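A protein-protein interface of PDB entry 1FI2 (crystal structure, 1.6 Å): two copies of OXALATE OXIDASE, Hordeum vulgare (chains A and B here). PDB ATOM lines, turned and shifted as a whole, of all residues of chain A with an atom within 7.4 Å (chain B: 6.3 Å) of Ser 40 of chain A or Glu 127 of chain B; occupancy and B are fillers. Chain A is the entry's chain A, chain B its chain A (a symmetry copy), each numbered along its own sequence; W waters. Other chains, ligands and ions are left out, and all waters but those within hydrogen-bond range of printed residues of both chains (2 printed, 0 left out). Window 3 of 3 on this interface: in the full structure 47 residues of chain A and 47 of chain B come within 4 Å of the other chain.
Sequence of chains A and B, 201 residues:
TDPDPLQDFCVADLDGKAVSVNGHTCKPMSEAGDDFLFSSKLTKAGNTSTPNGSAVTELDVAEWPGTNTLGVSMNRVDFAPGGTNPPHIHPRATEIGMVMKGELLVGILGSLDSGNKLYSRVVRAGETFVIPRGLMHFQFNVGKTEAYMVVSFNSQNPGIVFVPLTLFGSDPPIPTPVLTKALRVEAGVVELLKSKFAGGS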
ATOM      1  N   PHE A  38      22.821 -23.592  -2.259  1.00  0.00           N
ATOM      2  CA  PHE A  38      22.754 -24.047  -3.638  1.00  0.00           C
ATOM      3  C   PHE A  38      24.091 -23.959  -4.365  1.00  0.00           C
ATOM      4  O   PHE A  38      24.956 -23.154  -3.999  1.00  0.00           O
ATOM      5  CB  PHE A  38      21.717 -23.184  -4.390  1.00  0.00           C
ATOM      6  CG  PHE A  38      20.344 -23.200  -3.776  1.00  0.00           C
ATOM      7  CD1 PHE A  38      19.931 -22.169  -2.945  1.00  0.00           C
ATOM      8  CD2 PHE A  38      19.493 -24.273  -3.985  1.00  0.00           C
ATOM      9  CE1 PHE A  38      18.680 -22.186  -2.360  1.00  0.00           C
ATOM     10  CE2 PHE A  38      18.242 -24.294  -3.396  1.00  0.00           C
ATOM     11  CZ  PHE A  38      17.838 -23.256  -2.581  1.00  0.00           C
ATOM     12  N   SER A  39      24.272 -24.753  -5.421  1.00  0.00           N
ATOM     13  CA  SER A  39      25.473 -24.682  -6.243  1.00  0.00           C
ATOM     14  C   SER A  39      25.234 -25.206  -7.656  1.00  0.00           C
ATOM     15  O   SER A  39      24.292 -25.958  -7.908  1.00  0.00           O
ATOM     16  CB  SER A  39      26.634 -25.476  -5.631  1.00  0.00           C
ATOM     17  OG  SER A  39      27.800 -25.351  -6.437  1.00  0.00           O
ATOM     18  N   SER A  40      26.023 -24.698  -8.598  1.00  0.00           N
ATOM     19  CA  SER A  40      25.935 -25.159  -9.979  1.00  0.00           C
ATOM     20  C   SER A  40      27.301 -25.639 -10.460  1.00  0.00           C
ATOM     21  O   SER A  40      27.489 -25.872 -11.655  1.00  0.00           O
ATOM     22  CB  SER A  40      25.443 -24.038 -10.899  1.00  0.00           C
ATOM     23  OG  SER A  40      26.478 -23.076 -11.036  1.00  0.00           O
ATOM     24  N   LYS A  41      28.229 -25.855  -9.530  1.00  0.00           N
ATOM     25  CA  LYS A  41      29.579 -26.274  -9.885  1.00  0.00           C
ATOM     26  C   LYS A  41      29.700 -27.665 -10.482  1.00  0.00           C
ATOM     27  O   LYS A  41      30.710 -27.918 -11.159  1.00  0.00           O
ATOM     28  CB  LYS A  41      30.527 -26.115  -8.682  1.00  0.00           C
ATOM     29  CG  LYS A  41      30.818 -24.661  -8.343  1.00  0.00           C
ATOM     30  CD  LYS A  41      31.808 -24.506  -7.199  1.00  0.00           C
ATOM     31  CE  LYS A  41      32.197 -23.051  -6.999  1.00  0.00           C
ATOM     32  NZ  LYS A  41      33.147 -22.862  -5.867  1.00  0.00           N
ATOM     33  N   LEU A  42      28.725 -28.555 -10.328  1.00  0.00           N
ATOM     34  CA  LEU A  42      28.802 -29.884 -10.919  1.00  0.00           C
ATOM     35  C   LEU A  42      27.993 -30.020 -12.199  1.00  0.00           C
ATOM     36  O   LEU A  42      27.796 -31.133 -12.698  1.00  0.00           O
ATOM     37  CB  LEU A  42      28.346 -30.944  -9.904  1.00  0.00           C
ATOM     38  CG  LEU A  42      29.052 -30.929  -8.547  1.00  0.00           C
ATOM     39  CD1 LEU A  42      28.551 -32.066  -7.664  1.00  0.00           C
ATOM     40  CD2 LEU A  42      30.564 -31.013  -8.694  1.00  0.00           C
ATOM     41  N   THR A  43      27.523 -28.910 -12.768  1.00  0.00           N
ATOM     42  CA  THR A  43      26.740 -28.946 -13.989  1.00  0.00           C
ATOM     43  C   THR A  43      27.532 -29.407 -15.210  1.00  0.00           C
ATOM     44  O   THR A  43      26.923 -30.011 -16.099  1.00  0.00           O
ATOM     45  CB  THR A  43      26.105 -27.587 -14.351  1.00  0.00           C
ATOM     46  OG1 THR A  43      27.118 -26.572 -14.431  1.00  0.00           O
ATOM     47  CG2 THR A  43      25.052 -27.169 -13.343  1.00  0.00           C
ATOM     48  N   LYS A  44      28.815 -29.088 -15.304  1.00  0.00           N
ATOM     49  CA  LYS A  44      29.598 -29.439 -16.481  1.00  0.00           C
ATOM     50  C   LYS A  44      30.645 -30.515 -16.225  1.00  0.00           C
ATOM     51  O   LYS A  44      31.145 -30.710 -15.119  1.00  0.00           O
ATOM     52  CB  LYS A  44      30.283 -28.193 -17.058  1.00  0.00           C
ATOM     53  CG  LYS A  44      29.327 -27.077 -17.440  1.00  0.00           C
ATOM     54  CD  LYS A  44      30.037 -25.896 -18.083  1.00  0.00           C
ATOM     55  CE  LYS A  44      29.040 -24.802 -18.437  1.00  0.00           C
ATOM     56  NZ  LYS A  44      29.683 -23.674 -19.167  1.00  0.00           N
ATOM     57  N   LEU A  59      33.191 -30.808  -4.595  1.00  0.00           N
ATOM     58  CA  LEU A  59      32.154 -29.952  -4.022  1.00  0.00           C
ATOM     59  C   LEU A  59      32.124 -30.133  -2.506  1.00  0.00           C
ATOM     60  O   LEU A  59      31.100 -30.391  -1.879  1.00  0.00           O
ATOM     61  CB  LEU A  59      30.793 -30.180  -4.669  1.00  0.00           C
ATOM     62  CG  LEU A  59      29.817 -29.006  -4.617  1.00  0.00           C
ATOM     63  CD1 LEU A  59      30.397 -27.758  -5.268  1.00  0.00           C
ATOM     64  CD2 LEU A  59      28.495 -29.367  -5.286  1.00  0.00           C
ATOM     65  N   TRP A  64      32.049 -25.374  -1.665  1.00  0.00           N
ATOM     66  CA  TRP A  64      30.657 -25.116  -1.308  1.00  0.00           C
ATOM     67  C   TRP A  64      30.599 -24.802   0.183  1.00  0.00           C
ATOM     68  O   TRP A  64      30.320 -25.669   1.015  1.00  0.00           O
ATOM     69  CB  TRP A  64      29.776 -26.319  -1.625  1.00  0.00           C
ATOM     70  CG  TRP A  64      28.294 -26.111  -1.651  1.00  0.00           C
ATOM     71  CD1 TRP A  64      27.605 -24.940  -1.507  1.00  0.00           C
ATOM     72  CD2 TRP A  64      27.302 -27.114  -1.919  1.00  0.00           C
ATOM     73  NE1 TRP A  64      26.255 -25.156  -1.626  1.00  0.00           N
ATOM     74  CE2 TRP A  64      26.043 -26.484  -1.894  1.00  0.00           C
ATOM     75  CE3 TRP A  64      27.360 -28.491  -2.163  1.00  0.00           C
ATOM     76  CZ2 TRP A  64      24.850 -27.175  -2.102  1.00  0.00           C
ATOM     77  CZ3 TRP A  64      26.178 -29.177  -2.374  1.00  0.00           C
ATOM     78  CH2 TRP A  64      24.943 -28.518  -2.343  1.00  0.00           C
ATOM     79  N   MET A  74      29.648 -33.327  -1.752  1.00  0.00           N
ATOM     80  CA  MET A  74      29.548 -34.135  -2.956  1.00  0.00           C
ATOM     81  C   MET A  74      30.771 -33.955  -3.855  1.00  0.00           C
ATOM     82  O   MET A  74      31.648 -33.132  -3.620  1.00  0.00           O
ATOM     83  CB  MET A  74      28.350 -33.724  -3.821  1.00  0.00           C
ATOM     84  CG  MET A  74      26.968 -33.999  -3.275  1.00  0.00           C
ATOM     85  SD  MET A  74      25.690 -33.167  -4.235  1.00  0.00           S
ATOM     86  CE  MET A  74      25.340 -34.384  -5.481  1.00  0.00           C
ATOM     87  N   GLY B  97      21.191 -32.932  -2.413  1.00  0.00           N
ATOM     88  CA  GLY B  97      20.658 -33.491  -3.649  1.00  0.00           C
ATOM     89  C   GLY B  97      21.072 -32.808  -4.936  1.00  0.00           C
ATOM     90  O   GLY B  97      21.646 -31.723  -4.947  1.00  0.00           O
ATOM     91  N   MET B  98      20.775 -33.488  -6.044  1.00  0.00           N
ATOM     92  CA  MET B  98      21.077 -32.971  -7.371  1.00  0.00           C
ATOM     93  C   MET B  98      19.853 -33.151  -8.270  1.00  0.00           C
ATOM     94  O   MET B  98      19.265 -34.232  -8.275  1.00  0.00           O
ATOM     95  CB  MET B  98      22.297 -33.648  -8.007  1.00  0.00           C
ATOM     96  CG  MET B  98      22.608 -33.059  -9.381  1.00  0.00           C
ATOM     97  SD  MET B  98      23.958 -33.878 -10.245  1.00  0.00           S
ATOM     98  CE  MET B  98      25.370 -33.069  -9.507  1.00  0.00           C
ATOM     99  N   VAL B  99      19.500 -32.110  -9.017  1.00  0.00           N
ATOM    100  CA  VAL B  99      18.401 -32.247  -9.981  1.00  0.00           C
ATOM    101  C   VAL B  99      18.964 -32.906 -11.237  1.00  0.00           C
ATOM    102  O   VAL B  99      20.001 -32.470 -11.739  1.00  0.00           O
ATOM    103  CB  VAL B  99      17.761 -30.890 -10.295  1.00  0.00           C
ATOM    104  CG1 VAL B  99      16.814 -30.955 -11.489  1.00  0.00           C
ATOM    105  CG2 VAL B  99      17.003 -30.391  -9.069  1.00  0.00           C
ATOM    106  N   MET B 100      18.305 -33.955 -11.711  1.00  0.00           N
ATOM    107  CA  MET B 100      18.790 -34.658 -12.893  1.00  0.00           C
ATOM    108  C   MET B 100      18.136 -34.183 -14.179  1.00  0.00           C
ATOM    109  O   MET B 100      18.783 -34.151 -15.227  1.00  0.00           O
ATOM    110  CB  MET B 100      18.609 -36.163 -12.713  1.00  0.00           C
ATOM    111  CG  MET B 100      19.473 -36.790 -11.635  1.00  0.00           C
ATOM    112  SD  MET B 100      21.218 -36.392 -11.720  1.00  0.00           S
ATOM    113  CE  MET B 100      21.536 -36.280 -13.480  1.00  0.00           C
ATOM    114  N   VAL B 122      15.022 -21.813  -8.269  1.00  0.00           N
ATOM    115  CA  VAL B 122      14.711 -22.785  -9.321  1.00  0.00           C
ATOM    116  C   VAL B 122      16.017 -23.524  -9.630  1.00  0.00           C
ATOM    117  O   VAL B 122      17.013 -22.893  -9.978  1.00  0.00           O
ATOM    118  CB  VAL B 122      14.133 -22.146 -10.586  1.00  0.00           C
ATOM    119  CG1 VAL B 122      13.879 -23.184 -11.670  1.00  0.00           C
ATOM    120  CG2 VAL B 122      12.840 -21.409 -10.246  1.00  0.00           C
ATOM    121  N   VAL B 123      16.044 -24.819  -9.348  1.00  0.00           N
ATOM    122  CA  VAL B 123      17.225 -25.655  -9.525  1.00  0.00           C
ATOM    123  C   VAL B 123      17.075 -26.509 -10.775  1.00  0.00           C
ATOM    124  O   VAL B 123      16.046 -27.165 -10.961  1.00  0.00           O
ATOM    125  CB  VAL B 123      17.447 -26.547  -8.289  1.00  0.00           C
ATOM    126  CG1 VAL B 123      18.714 -27.382  -8.413  1.00  0.00           C
ATOM    127  CG2 VAL B 123      17.512 -25.709  -7.017  1.00  0.00           C
ATOM    128  N   ARG B 124      18.071 -26.476 -11.664  1.00  0.00           N
ATOM    129  CA  ARG B 124      17.993 -27.218 -12.922  1.00  0.00           C
ATOM    130  C   ARG B 124      19.009 -28.342 -13.032  1.00  0.00           C
ATOM    131  O   ARG B 124      19.759 -28.600 -12.091  1.00  0.00           O
ATOM    132  CB  ARG B 124      18.112 -26.226 -14.095  1.00  0.00           C
ATOM    133  CG  ARG B 124      16.969 -25.225 -14.114  1.00  0.00           C
ATOM    134  CD  ARG B 124      16.930 -24.318 -15.326  1.00  0.00           C
ATOM    135  NE  ARG B 124      15.840 -23.348 -15.218  1.00  0.00           N
ATOM    136  CZ  ARG B 124      15.884 -22.195 -14.569  1.00  0.00           C
ATOM    137  NH1 ARG B 124      16.991 -21.803 -13.949  1.00  0.00           N
ATOM    138  NH2 ARG B 124      14.816 -21.402 -14.534  1.00  0.00           N
ATOM    139  N   ALA B 125      19.016 -29.055 -14.157  1.00  0.00           N
ATOM    140  CA  ALA B 125      19.895 -30.200 -14.352  1.00  0.00           C
ATOM    141  C   ALA B 125      21.344 -29.957 -13.965  1.00  0.00           C
ATOM    142  O   ALA B 125      22.001 -29.025 -14.423  1.00  0.00           O
ATOM    143  CB  ALA B 125      19.835 -30.664 -15.807  1.00  0.00           C
ATOM    144  N   GLY B 126      21.872 -30.813 -13.087  1.00  0.00           N
ATOM    145  CA  GLY B 126      23.235 -30.735 -12.612  1.00  0.00           C
ATOM    146  C   GLY B 126      23.462 -29.803 -11.431  1.00  0.00           C
ATOM    147  O   GLY B 126      24.566 -29.775 -10.878  1.00  0.00           O
ATOM    148  N   GLU B 127      22.452 -29.034 -11.049  1.00  0.00           N
ATOM    149  CA  GLU B 127      22.574 -28.100  -9.933  1.00  0.00           C
ATOM    150  C   GLU B 127      22.196 -28.792  -8.632  1.00  0.00           C
ATOM    151  O   GLU B 127      21.371 -29.711  -8.631  1.00  0.00           O
ATOM    152  CB  GLU B 127      21.727 -26.859 -10.206  1.00  0.00           C
ATOM    153  CG  GLU B 127      22.070 -26.194 -11.540  1.00  0.00           C
ATOM    154  CD  GLU B 127      21.435 -24.823 -11.661  1.00  0.00           C
ATOM    155  OE1 GLU B 127      20.220 -24.692 -11.415  1.00  0.00           O
ATOM    156  OE2 GLU B 127      22.153 -23.855 -11.994  1.00  0.00           O
ATOM    157  N   THR B 128      22.813 -28.377  -7.531  1.00  0.00           N
ATOM    158  CA  THR B 128      22.603 -29.031  -6.242  1.00  0.00           C
ATOM    159  C   THR B 128      22.048 -28.127  -5.152  1.00  0.00           C
ATOM    160  O   THR B 128      22.078 -26.902  -5.239  1.00  0.00           O
ATOM    161  CB  THR B 128      23.945 -29.615  -5.734  1.00  0.00           C
ATOM    162  OG1 THR B 128      24.918 -28.562  -5.727  1.00  0.00           O
ATOM    163  CG2 THR B 128      24.448 -30.747  -6.617  1.00  0.00           C
ATOM    164  N   PHE B 129      21.550 -28.770  -4.095  1.00  0.00           N
ATOM    165  CA  PHE B 129      20.973 -28.093  -2.946  1.00  0.00           C
ATOM    166  C   PHE B 129      21.271 -28.855  -1.654  1.00  0.00           C
ATOM    167  O   PHE B 129      21.551 -30.052  -1.679  1.00  0.00           O
ATOM    168  CB  PHE B 129      19.456 -27.946  -3.097  1.00  0.00           C
ATOM    169  CG  PHE B 129      18.676 -29.219  -3.253  1.00  0.00           C
ATOM    170  CD1 PHE B 129      18.250 -29.943  -2.152  1.00  0.00           C
ATOM    171  CD2 PHE B 129      18.349 -29.692  -4.514  1.00  0.00           C
ATOM    172  CE1 PHE B 129      17.528 -31.109  -2.305  1.00  0.00           C
ATOM    173  CE2 PHE B 129      17.625 -30.860  -4.679  1.00  0.00           C
ATOM    174  CZ  PHE B 129      17.217 -31.570  -3.567  1.00  0.00           C
HETATM  175  O   HOH W   1      26.116 -28.381  -8.986  1.00  0.00           O
HETATM  176  O   HOH W   2      23.966 -30.063 -16.561  1.00  0.00           O
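Printed residues of chain B that touch a printed residue of chain A: Met 98, Val 123, Ala 125, Gly 126, Glu 127, Thr 128 and Phe 129.
Hydrophobic or aromatic side chains of chain B that line the printed part of chain A: Met 98, Val 123 and Phe 129.
Of the 10 printed residues of chain A, 8 touch a printed residue of chain B.
Hydrophobic or aromatic side chains of chain A that line the printed part of chain B: Phe 38, Leu 42, Leu 59, Trp 64 and Met 74.
Among the printed residues, 15 pairs touch across the chains.
Among the printed residues, no Asp or Glu carboxylate lies within 4 Å of a Lys or Arg side-chain nitrogen of the other chain.
No position is printed for both chains.
Of the 15 pairs that touch across the chains among the printed residues, none has its exchanged pair printed and touching as well.
O of Phe 38 of chain A lies within hydrogen-bond range of NE1 of Trp 64 of chain A (3.4 Å).
The backbone carbonyl oxygen (O) of Ser 40 of chain A lies within hydrogen-bond range of the side-chain hydroxyl (OG1) of Thr 43 of chain A (2.9 Å).
O of Phe 129 of chain B lies within hydrogen-bond range of N of Gly 97 of chain B (3.0 Å).
The backbone carbonyl oxygen of Val 99 of chain B lies within hydrogen-bond range of the backbone NH of Gly 126 of chain B.
The backbone NH of Val 99 of chain B sits at hydrogen-bond distance from the backbone carbonyl oxygen of Glu 127 of chain B (3.1 Å).
The side-chain carboxylate (OE1) of Glu 127 of chain B is in hydrogen-bond range of the backbone NH (N) of Arg 124 of chain B (2.8 Å).
Water W1 lies within hydrogen-bond range of O of Gly 126 of chain B (2.8 Å), N of Leu 42 of chain A (2.9 Å), O of Ser 39 of chain A (3.2 Å), N of Lys 41 of chain A (3.3 Å) and OG1 of Thr 128 of chain B (3.5 Å).
Water W2 lies within hydrogen-bond range of O of Thr 43 of chain A (3.0 Å) and O of Ala 125 of chain B (3.1 Å).
The backbone NH (N) of Thr 128 of chain B is in hydrogen-bond range of the backbone carbonyl oxygen (O) of Ser 39 of chain A (2.9 Å).
Phe 38 of chain A touches Val 123 of chain B (CD2 to CG2, 3.9 Å).
CA of Phe 38 of chain A touches O of Thr 128 of chain B (3.3 Å).
CB of Phe 129 of chain B touches CD2 of Phe 38 of chain A (3.8 Å).
CA of Glu 127 of chain B touches O of Ser 39 of chain A (3.4 Å).
Ser 40 of chain A touches Glu 127 of chain B (CB to OE2, 3.5 Å).
O of Gly 126 of chain B touches N of Thr 43 of chain A, 3.6 Å away.
Thr 43 of chain A touches Glu 127 of chain B.
Leu 59 of chain A touches Thr 128 of chain B (CD2 to OG1, 3.7 Å).
Phe 129 of chain B touches Trp 64 of chain A (C to CH2, 3.8 Å).
Thr 128 of chain B touches Met 74 of chain A (CG2 to SD, 3.6 Å).
Of chain B, only Glu 127 (3.5 Å) comes within 4 Å of Ser 40 of chain A.
Lys 41 of chain A touches none of the printed residues of chain B.
Printed residues of chain B within 4 Å of Leu 42 of chain A: Met 98 and Gly 126.
Of the printed residues of chain B, Met 74 of chain A touches Thr 128 (3.6 Å).
Printed residues of chain A within 4 Å of Phe 129 of chain B: Phe 38 and Trp 64.
The nearest residue of chain B that does not touch Ser 40 of chain A is Gly 126 of chain B (4.9 Å).
The nearest printed residue of chain A that does not touch Met 98 of chain B is Met 74 of chain A (4.02 Å).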
